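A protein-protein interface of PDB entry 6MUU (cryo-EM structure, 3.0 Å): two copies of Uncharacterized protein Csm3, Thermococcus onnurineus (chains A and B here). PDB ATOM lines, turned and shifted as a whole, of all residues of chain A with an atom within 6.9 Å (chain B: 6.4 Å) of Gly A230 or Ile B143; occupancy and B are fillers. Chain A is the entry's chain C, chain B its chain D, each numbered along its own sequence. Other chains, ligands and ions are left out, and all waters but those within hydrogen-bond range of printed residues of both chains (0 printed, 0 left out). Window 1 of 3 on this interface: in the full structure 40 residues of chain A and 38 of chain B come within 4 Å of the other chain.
The backbone carbonyl oxygen of Ser A224 sits at hydrogen-bond distance from the guanidinium group of Arg B145 (3.4 Å). NZ of Lys A236 is in salt-bridge range of OE1 of Glu B196 (3.3 Å). O of Val B144 lies close to N of Gly A233 (3.3 Å). OG of Ser A231 lies within hydrogen-bond range of O of Ile B142. O of Asp A223 lies within hydrogen-bond range of NH1 of Arg B145 (3.0 Å). The side-chain hydroxyl (OG) of Ser A231 lies close to the side-chain hydroxyl (OG) of Ser B140 (3.4 Å). O of Ser A231 is in hydrogen-bond range of N of Val B144, at 3.2 Å.
O of Ile B143 is in hydrogen-bond range of N of Ile B198 (3.0 Å). The side-chain carboxylate of Glu B196 is in salt-bridge range of the guanidinium group of Arg B145 (3.98 Å). N of Ile B142 is in hydrogen-bond range of OG of Ser B140 (2.9 Å). The guanidinium group (NH1) of Arg A232 is in hydrogen-bond range of the side-chain hydroxyl (OG) of Ser A229, at 3.4 Å. The backbone carbonyl oxygen (O) of Tyr A225 is in hydrogen-bond range of the guanidinium group (NH2) of Arg A59, 2.4 Å away.
Among the printed residues, merely in contact across the chains: Gly A230 with Ile B143 (3.3 Å), Asp A223 with Ile B198 (3.5 Å), Arg A232 with Val B144 (3.5 Å), Lys A236 with Arg B145 (3.5 Å), Asp A223 with Lys B9 (3.6 Å), Asp A223 with Ile B143 (3.8 Å), Ser A231 with Ile B143 (3.9 Å), Ser A224 with Ile B143 (3.9 Å), Gly A233 with Arg B145 (3.9 Å) and Tyr A225 with Ile B143 (3.98 Å).
Gly A230 touches just one residue of chain B: Ile B143 (3.3 Å). Of chain A, only Asp A223 (3.8 Å), Ser A224 (3.9 Å), Tyr A225 (3.98 Å), Gly A230 (3.3 Å) and Ser A231 (3.9 Å) come within 4 Å of Ile B143. Of the printed residues of chain A, Val B144 touches Ser A231, Arg A232 and Gly A233. Of the printed residues of chain A, Arg B145 touches Asp A223 (3.0 Å), Ser A224 (3.4 Å), Gly A233 (3.9 Å) and Lys A236 (3.5 Å). Tyr A234 touches none of the printed residues of chain B. Arg B141 touches none of the printed residues of chain A. The nearest residue of chain A that does not touch Ile B143 is Gly A233 (4.8 Å).
Of the 15 printed residues of chain A, 8 touch a printed residue of chain B. Printed residues of chain A that touch a printed residue of chain B: Asp A223, Ser A224, Tyr A225, Gly A230, Ser A231, Arg A232, Gly A233 and Lys A236. Printed residues of chain B that touch a printed residue of chain A: Lys B9, Ser B140, Ile B142, Ile B143, Val B144, Arg B145, Glu B196 and Ile B198. Hydrophobic or aromatic side chains of chain B that line the printed part of chain A: Ile B143 and Ile B198.
No position is printed for both chains. Of the 17 pairs that touch across the chains among the printed residues, none has its exchanged pair printed and touching as well.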
ATOM      1  N   ARG A  59       5.679  24.446 -11.974  1.00  0.00           N
ATOM      2  CA  ARG A  59       6.127  24.030 -10.656  1.00  0.00           C
ATOM      3  C   ARG A  59       7.591  24.377 -10.436  1.00  0.00           C
ATOM      4  O   ARG A  59       7.963  24.804  -9.339  1.00  0.00           O
ATOM      5  CB  ARG A  59       5.894  22.538 -10.436  1.00  0.00           C
ATOM      6  CG  ARG A  59       6.212  22.144  -9.012  1.00  0.00           C
ATOM      7  CD  ARG A  59       5.248  22.877  -8.117  1.00  0.00           C
ATOM      8  NE  ARG A  59       5.635  22.941  -6.718  1.00  0.00           N
ATOM      9  CZ  ARG A  59       5.322  22.034  -5.813  1.00  0.00           C
ATOM     10  NH1 ARG A  59       5.711  22.193  -4.561  1.00  0.00           N
ATOM     11  NH2 ARG A  59       4.640  20.959  -6.167  1.00  0.00           N
ATOM     12  N   ASP A 223      11.994  16.548  -3.650  1.00  0.00           N
ATOM     13  CA  ASP A 223      11.580  16.504  -2.258  1.00  0.00           C
ATOM     14  C   ASP A 223      10.221  17.140  -2.013  1.00  0.00           C
ATOM     15  O   ASP A 223       9.623  16.889  -0.964  1.00  0.00           O
ATOM     16  CB  ASP A 223      12.621  17.180  -1.369  1.00  0.00           C
ATOM     17  CG  ASP A 223      13.845  16.319  -1.147  1.00  0.00           C
ATOM     18  OD1 ASP A 223      13.708  15.080  -1.162  1.00  0.00           O
ATOM     19  OD2 ASP A 223      14.940  16.877  -0.943  1.00  0.00           O
ATOM     20  N   SER A 224       9.735  17.969  -2.927  1.00  0.00           N
ATOM     21  CA  SER A 224       8.338  18.373  -2.928  1.00  0.00           C
ATOM     22  C   SER A 224       7.570  17.432  -3.853  1.00  0.00           C
ATOM     23  O   SER A 224       8.052  16.350  -4.195  1.00  0.00           O
ATOM     24  CB  SER A 224       8.198  19.838  -3.328  1.00  0.00           C
ATOM     25  OG  SER A 224       8.559  20.018  -4.675  1.00  0.00           O
ATOM     26  N   TYR A 225       6.367  17.811  -4.243  1.00  0.00           N
ATOM     27  CA  TYR A 225       5.518  16.989  -5.082  1.00  0.00           C
ATOM     28  C   TYR A 225       5.260  17.695  -6.409  1.00  0.00           C
ATOM     29  O   TYR A 225       5.676  18.831  -6.622  1.00  0.00           O
ATOM     30  CB  TYR A 225       4.219  16.657  -4.347  1.00  0.00           C
ATOM     31  CG  TYR A 225       3.359  17.837  -3.974  1.00  0.00           C
ATOM     32  CD1 TYR A 225       3.571  18.531  -2.790  1.00  0.00           C
ATOM     33  CD2 TYR A 225       2.300  18.221  -4.776  1.00  0.00           C
ATOM     34  CE1 TYR A 225       2.789  19.590  -2.447  1.00  0.00           C
ATOM     35  CE2 TYR A 225       1.502  19.270  -4.430  1.00  0.00           C
ATOM     36  CZ  TYR A 225       1.752  19.951  -3.266  1.00  0.00           C
ATOM     37  OH  TYR A 225       0.951  21.008  -2.925  1.00  0.00           O
ATOM     38  N   LEU A 226       4.572  17.001  -7.310  1.00  0.00           N
ATOM     39  CA  LEU A 226       4.206  17.535  -8.617  1.00  0.00           C
ATOM     40  C   LEU A 226       2.721  17.311  -8.836  1.00  0.00           C
ATOM     41  O   LEU A 226       2.301  16.186  -9.113  1.00  0.00           O
ATOM     42  CB  LEU A 226       5.007  16.876  -9.733  1.00  0.00           C
ATOM     43  CG  LEU A 226       4.638  17.318 -11.149  1.00  0.00           C
ATOM     44  CD1 LEU A 226       4.991  18.767 -11.375  1.00  0.00           C
ATOM     45  CD2 LEU A 226       5.300  16.433 -12.169  1.00  0.00           C
ATOM     46  N   GLY A 227       1.928  18.368  -8.708  1.00  0.00           N
ATOM     47  CA  GLY A 227       0.509  18.297  -8.979  1.00  0.00           C
ATOM     48  C   GLY A 227      -0.312  17.519  -7.971  1.00  0.00           C
ATOM     49  O   GLY A 227       0.213  16.686  -7.233  1.00  0.00           O
ATOM     50  N   GLY A 228      -1.610  17.776  -7.928  1.00  0.00           N
ATOM     51  CA  GLY A 228      -2.490  16.939  -7.145  1.00  0.00           C
ATOM     52  C   GLY A 228      -2.364  17.191  -5.659  1.00  0.00           C
ATOM     53  O   GLY A 228      -1.920  18.246  -5.228  1.00  0.00           O
ATOM     54  N   SER A 229      -2.701  16.166  -4.878  1.00  0.00           N
ATOM     55  CA  SER A 229      -2.855  16.341  -3.440  1.00  0.00           C
ATOM     56  C   SER A 229      -1.519  16.552  -2.750  1.00  0.00           C
ATOM     57  O   SER A 229      -1.346  17.527  -2.012  1.00  0.00           O
ATOM     58  CB  SER A 229      -3.585  15.143  -2.847  1.00  0.00           C
ATOM     59  OG  SER A 229      -4.904  15.073  -3.351  1.00  0.00           O
ATOM     60  N   GLY A 230      -0.573  15.652  -2.947  1.00  0.00           N
ATOM     61  CA  GLY A 230       0.794  15.932  -2.562  1.00  0.00           C
ATOM     62  C   GLY A 230       1.128  15.969  -1.086  1.00  0.00           C
ATOM     63  O   GLY A 230       2.025  15.256  -0.638  1.00  0.00           O
ATOM     64  N   SER A 231       0.444  16.826  -0.326  1.00  0.00           N
ATOM     65  CA  SER A 231       0.550  16.791   1.126  1.00  0.00           C
ATOM     66  C   SER A 231      -0.004  15.492   1.688  1.00  0.00           C
ATOM     67  O   SER A 231       0.462  15.016   2.727  1.00  0.00           O
ATOM     68  CB  SER A 231      -0.178  17.986   1.731  1.00  0.00           C
ATOM     69  OG  SER A 231      -0.125  17.949   3.143  1.00  0.00           O
ATOM     70  N   ARG A 232      -0.979  14.902   1.013  1.00  0.00           N
ATOM     71  CA  ARG A 232      -1.422  13.546   1.268  1.00  0.00           C
ATOM     72  C   ARG A 232      -0.562  12.500   0.571  1.00  0.00           C
ATOM     73  O   ARG A 232      -0.969  11.340   0.495  1.00  0.00           O
ATOM     74  CB  ARG A 232      -2.878  13.383   0.836  1.00  0.00           C
ATOM     75  CG  ARG A 232      -3.904  13.806   1.876  1.00  0.00           C
ATOM     76  CD  ARG A 232      -4.222  15.272   1.827  1.00  0.00           C
ATOM     77  NE  ARG A 232      -4.959  15.657   0.637  1.00  0.00           N
ATOM     78  CZ  ARG A 232      -5.067  16.908   0.220  1.00  0.00           C
ATOM     79  NH1 ARG A 232      -5.752  17.182  -0.876  1.00  0.00           N
ATOM     80  NH2 ARG A 232      -4.468  17.876   0.885  1.00  0.00           N
ATOM     81  N   GLY A 233       0.601  12.876   0.057  1.00  0.00           N
ATOM     82  CA  GLY A 233       1.512  11.951  -0.582  1.00  0.00           C
ATOM     83  C   GLY A 233       1.092  11.445  -1.940  1.00  0.00           C
ATOM     84  O   GLY A 233       0.769  10.265  -2.075  1.00  0.00           O
ATOM     85  N   TYR A 234       1.082  12.306  -2.955  1.00  0.00           N
ATOM     86  CA  TYR A 234       0.844  11.845  -4.313  1.00  0.00           C
ATOM     87  C   TYR A 234       2.053  11.988  -5.222  1.00  0.00           C
ATOM     88  O   TYR A 234       2.461  10.994  -5.820  1.00  0.00           O
ATOM     89  CB  TYR A 234      -0.339  12.554  -4.980  1.00  0.00           C
ATOM     90  CG  TYR A 234      -1.726  12.137  -4.549  1.00  0.00           C
ATOM     91  CD1 TYR A 234      -1.931  11.252  -3.515  1.00  0.00           C
ATOM     92  CD2 TYR A 234      -2.828  12.559  -5.266  1.00  0.00           C
ATOM     93  CE1 TYR A 234      -3.193  10.868  -3.148  1.00  0.00           C
ATOM     94  CE2 TYR A 234      -4.093  12.175  -4.912  1.00  0.00           C
ATOM     95  CZ  TYR A 234      -4.269  11.327  -3.855  1.00  0.00           C
ATOM     96  OH  TYR A 234      -5.535  10.936  -3.503  1.00  0.00           O
ATOM     97  N   GLY A 235       2.643  13.177  -5.345  1.00  0.00           N
ATOM     98  CA  GLY A 235       3.514  13.466  -6.473  1.00  0.00           C
ATOM     99  C   GLY A 235       4.779  12.646  -6.612  1.00  0.00           C
ATOM    100  O   GLY A 235       4.773  11.732  -7.437  1.00  0.00           O
ATOM    101  N   LYS A 236       5.795  12.902  -5.778  1.00  0.00           N
ATOM    102  CA  LYS A 236       7.003  12.080  -5.582  1.00  0.00           C
ATOM    103  C   LYS A 236       7.628  11.640  -6.915  1.00  0.00           C
ATOM    104  O   LYS A 236       7.527  10.498  -7.357  1.00  0.00           O
ATOM    105  CB  LYS A 236       6.670  10.912  -4.650  1.00  0.00           C
ATOM    106  CG  LYS A 236       7.809   9.991  -4.244  1.00  0.00           C
ATOM    107  CD  LYS A 236       8.857  10.657  -3.425  1.00  0.00           C
ATOM    108  CE  LYS A 236       9.873   9.642  -2.962  1.00  0.00           C
ATOM    109  NZ  LYS A 236      10.955  10.264  -2.162  1.00  0.00           N
ATOM    110  N   LYS B   9      14.352  21.581   4.347  1.00  0.00           N
ATOM    111  CA  LYS B   9      13.389  20.544   4.666  1.00  0.00           C
ATOM    112  C   LYS B   9      13.974  19.604   5.702  1.00  0.00           C
ATOM    113  O   LYS B   9      15.139  19.218   5.609  1.00  0.00           O
ATOM    114  CB  LYS B   9      13.003  19.747   3.428  1.00  0.00           C
ATOM    115  CG  LYS B   9      12.281  20.543   2.370  1.00  0.00           C
ATOM    116  CD  LYS B   9      11.911  19.655   1.218  1.00  0.00           C
ATOM    117  CE  LYS B   9      11.137  20.379   0.144  1.00  0.00           C
ATOM    118  NZ  LYS B   9      11.961  21.356  -0.596  1.00  0.00           N
ATOM    119  N   SER B 140       0.009  23.358   3.298  1.00  0.00           N
ATOM    120  CA  SER B 140       0.588  22.593   4.388  1.00  0.00           C
ATOM    121  C   SER B 140       2.091  22.783   4.460  1.00  0.00           C
ATOM    122  O   SER B 140       2.739  23.225   3.512  1.00  0.00           O
ATOM    123  CB  SER B 140       0.312  21.109   4.227  1.00  0.00           C
ATOM    124  OG  SER B 140       0.949  20.382   5.252  1.00  0.00           O
ATOM    125  N   ARG B 141       2.650  22.430   5.606  1.00  0.00           N
ATOM    126  CA  ARG B 141       4.088  22.396   5.745  1.00  0.00           C
ATOM    127  C   ARG B 141       4.635  20.985   5.796  1.00  0.00           C
ATOM    128  O   ARG B 141       5.855  20.820   5.827  1.00  0.00           O
ATOM    129  CB  ARG B 141       4.520  23.170   6.986  1.00  0.00           C
ATOM    130  CG  ARG B 141       4.348  24.657   6.852  1.00  0.00           C
ATOM    131  CD  ARG B 141       4.773  25.366   8.104  1.00  0.00           C
ATOM    132  NE  ARG B 141       4.613  26.806   7.974  1.00  0.00           N
ATOM    133  CZ  ARG B 141       4.846  27.666   8.954  1.00  0.00           C
ATOM    134  NH1 ARG B 141       5.235  27.224  10.138  1.00  0.00           N
ATOM    135  NH2 ARG B 141       4.680  28.965   8.756  1.00  0.00           N
ATOM    136  N   ILE B 142       3.783  19.961   5.785  1.00  0.00           N
ATOM    137  CA  ILE B 142       4.277  18.592   5.781  1.00  0.00           C
ATOM    138  C   ILE B 142       3.784  17.848   4.550  1.00  0.00           C
ATOM    139  O   ILE B 142       2.743  18.164   3.968  1.00  0.00           O
ATOM    140  CB  ILE B 142       3.909  17.806   7.055  1.00  0.00           C
ATOM    141  CG1 ILE B 142       2.406  17.635   7.183  1.00  0.00           C
ATOM    142  CG2 ILE B 142       4.476  18.481   8.276  1.00  0.00           C
ATOM    143  CD1 ILE B 142       2.046  16.611   8.203  1.00  0.00           C
ATOM    144  N   ILE B 143       4.574  16.860   4.148  1.00  0.00           N
ATOM    145  CA  ILE B 143       4.240  15.901   3.105  1.00  0.00           C
ATOM    146  C   ILE B 143       4.364  14.526   3.728  1.00  0.00           C
ATOM    147  O   ILE B 143       5.426  14.179   4.252  1.00  0.00           O
ATOM    148  CB  ILE B 143       5.174  16.021   1.895  1.00  0.00           C
ATOM    149  CG1 ILE B 143       5.004  17.365   1.206  1.00  0.00           C
ATOM    150  CG2 ILE B 143       4.917  14.909   0.919  1.00  0.00           C
ATOM    151  CD1 ILE B 143       6.055  17.626   0.181  1.00  0.00           C
ATOM    152  N   VAL B 144       3.296  13.748   3.683  1.00  0.00           N
ATOM    153  CA  VAL B 144       3.304  12.398   4.226  1.00  0.00           C
ATOM    154  C   VAL B 144       3.162  11.459   3.041  1.00  0.00           C
ATOM    155  O   VAL B 144       2.062  11.286   2.515  1.00  0.00           O
ATOM    156  CB  VAL B 144       2.191  12.183   5.253  1.00  0.00           C
ATOM    157  CG1 VAL B 144       2.258  10.784   5.803  1.00  0.00           C
ATOM    158  CG2 VAL B 144       2.306  13.193   6.368  1.00  0.00           C
ATOM    159  N   ARG B 145       4.268  10.849   2.622  1.00  0.00           N
ATOM    160  CA  ARG B 145       4.281  10.006   1.437  1.00  0.00           C
ATOM    161  C   ARG B 145       3.492   8.721   1.678  1.00  0.00           C
ATOM    162  O   ARG B 145       3.217   8.339   2.816  1.00  0.00           O
ATOM    163  CB  ARG B 145       5.712   9.637   1.054  1.00  0.00           C
ATOM    164  CG  ARG B 145       6.706  10.766   0.879  1.00  0.00           C
ATOM    165  CD  ARG B 145       6.457  11.614  -0.337  1.00  0.00           C
ATOM    166  NE  ARG B 145       7.607  12.469  -0.606  1.00  0.00           N
ATOM    167  CZ  ARG B 145       7.652  13.384  -1.563  1.00  0.00           C
ATOM    168  NH1 ARG B 145       8.746  14.096  -1.744  1.00  0.00           N
ATOM    169  NH2 ARG B 145       6.609  13.578  -2.348  1.00  0.00           N
ATOM    170  N   GLU B 196       7.713   8.206   5.060  1.00  0.00           N
ATOM    171  CA  GLU B 196       8.512   9.412   4.905  1.00  0.00           C
ATOM    172  C   GLU B 196       7.658  10.623   5.227  1.00  0.00           C
ATOM    173  O   GLU B 196       6.538  10.742   4.726  1.00  0.00           O
ATOM    174  CB  GLU B 196       9.063   9.518   3.486  1.00  0.00           C
ATOM    175  CG  GLU B 196       9.967  10.693   3.257  1.00  0.00           C
ATOM    176  CD  GLU B 196      10.489  10.733   1.840  1.00  0.00           C
ATOM    177  OE1 GLU B 196      10.112   9.852   1.041  1.00  0.00           O
ATOM    178  OE2 GLU B 196      11.283  11.637   1.517  1.00  0.00           O
ATOM    179  N   ILE B 197       8.178  11.507   6.076  1.00  0.00           N
ATOM    180  CA  ILE B 197       7.496  12.735   6.465  1.00  0.00           C
ATOM    181  C   ILE B 197       8.468  13.888   6.277  1.00  0.00           C
ATOM    182  O   ILE B 197       9.584  13.855   6.802  1.00  0.00           O
ATOM    183  CB  ILE B 197       6.986  12.667   7.914  1.00  0.00           C
ATOM    184  CG1 ILE B 197       5.934  11.569   8.046  1.00  0.00           C
ATOM    185  CG2 ILE B 197       6.361  13.966   8.306  1.00  0.00           C
ATOM    186  CD1 ILE B 197       5.598  11.200   9.437  1.00  0.00           C
ATOM    187  N   ILE B 198       8.051  14.901   5.526  1.00  0.00           N
ATOM    188  CA  ILE B 198       8.924  15.982   5.094  1.00  0.00           C
ATOM    189  C   ILE B 198       8.322  17.290   5.575  1.00  0.00           C
ATOM    190  O   ILE B 198       7.312  17.741   5.029  1.00  0.00           O
ATOM    191  CB  ILE B 198       9.089  16.000   3.570  1.00  0.00           C
ATOM    192  CG1 ILE B 198       9.654  14.677   3.073  1.00  0.00           C
ATOM    193  CG2 ILE B 198       9.994  17.124   3.152  1.00  0.00           C
ATOM    194  CD1 ILE B 198       9.617  14.539   1.592  1.00  0.00           C
ATOM    195  N   TYR B 199       8.940  17.912   6.572  1.00  0.00           N
ATOM    196  CA  TYR B 199       8.503  19.213   7.062  1.00  0.00           C
ATOM    197  C   TYR B 199       9.252  20.330   6.347  1.00  0.00           C
ATOM    198  O   TYR B 199      10.484  20.330   6.309  1.00  0.00           O
ATOM    199  CB  TYR B 199       8.719  19.316   8.571  1.00  0.00           C
ATOM    200  CG  TYR B 199       8.439  20.688   9.121  1.00  0.00           C
ATOM    201  CD1 TYR B 199       7.151  21.171   9.204  1.00  0.00           C
ATOM    202  CD2 TYR B 199       9.471  21.498   9.561  1.00  0.00           C
ATOM    203  CE1 TYR B 199       6.899  22.426   9.685  1.00  0.00           C
ATOM    204  CE2 TYR B 199       9.228  22.752  10.052  1.00  0.00           C
ATOM    205  CZ  TYR B 199       7.941  23.211  10.110  1.00  0.00           C
ATOM    206  OH  TYR B 199       7.690  24.467  10.608  1.00  0.00           O
ATOM    207  N   ASN B 200       8.507  21.285   5.798  1.00  0.00           N
ATOM    208  CA  ASN B 200       9.082  22.452   5.138  1.00  0.00           C
ATOM    209  C   ASN B 200       9.380  23.535   6.164  1.00  0.00           C
ATOM    210  O   ASN B 200       8.462  24.042   6.813  1.00  0.00           O
ATOM    211  CB  ASN B 200       8.131  23.010   4.086  1.00  0.00           C
ATOM    212  CG  ASN B 200       8.082  22.173   2.847  1.00  0.00           C
ATOM    213  OD1 ASN B 200       9.112  21.754   2.334  1.00  0.00           O
ATOM    214  ND2 ASN B 200       6.881  21.913   2.355  1.00  0.00           N
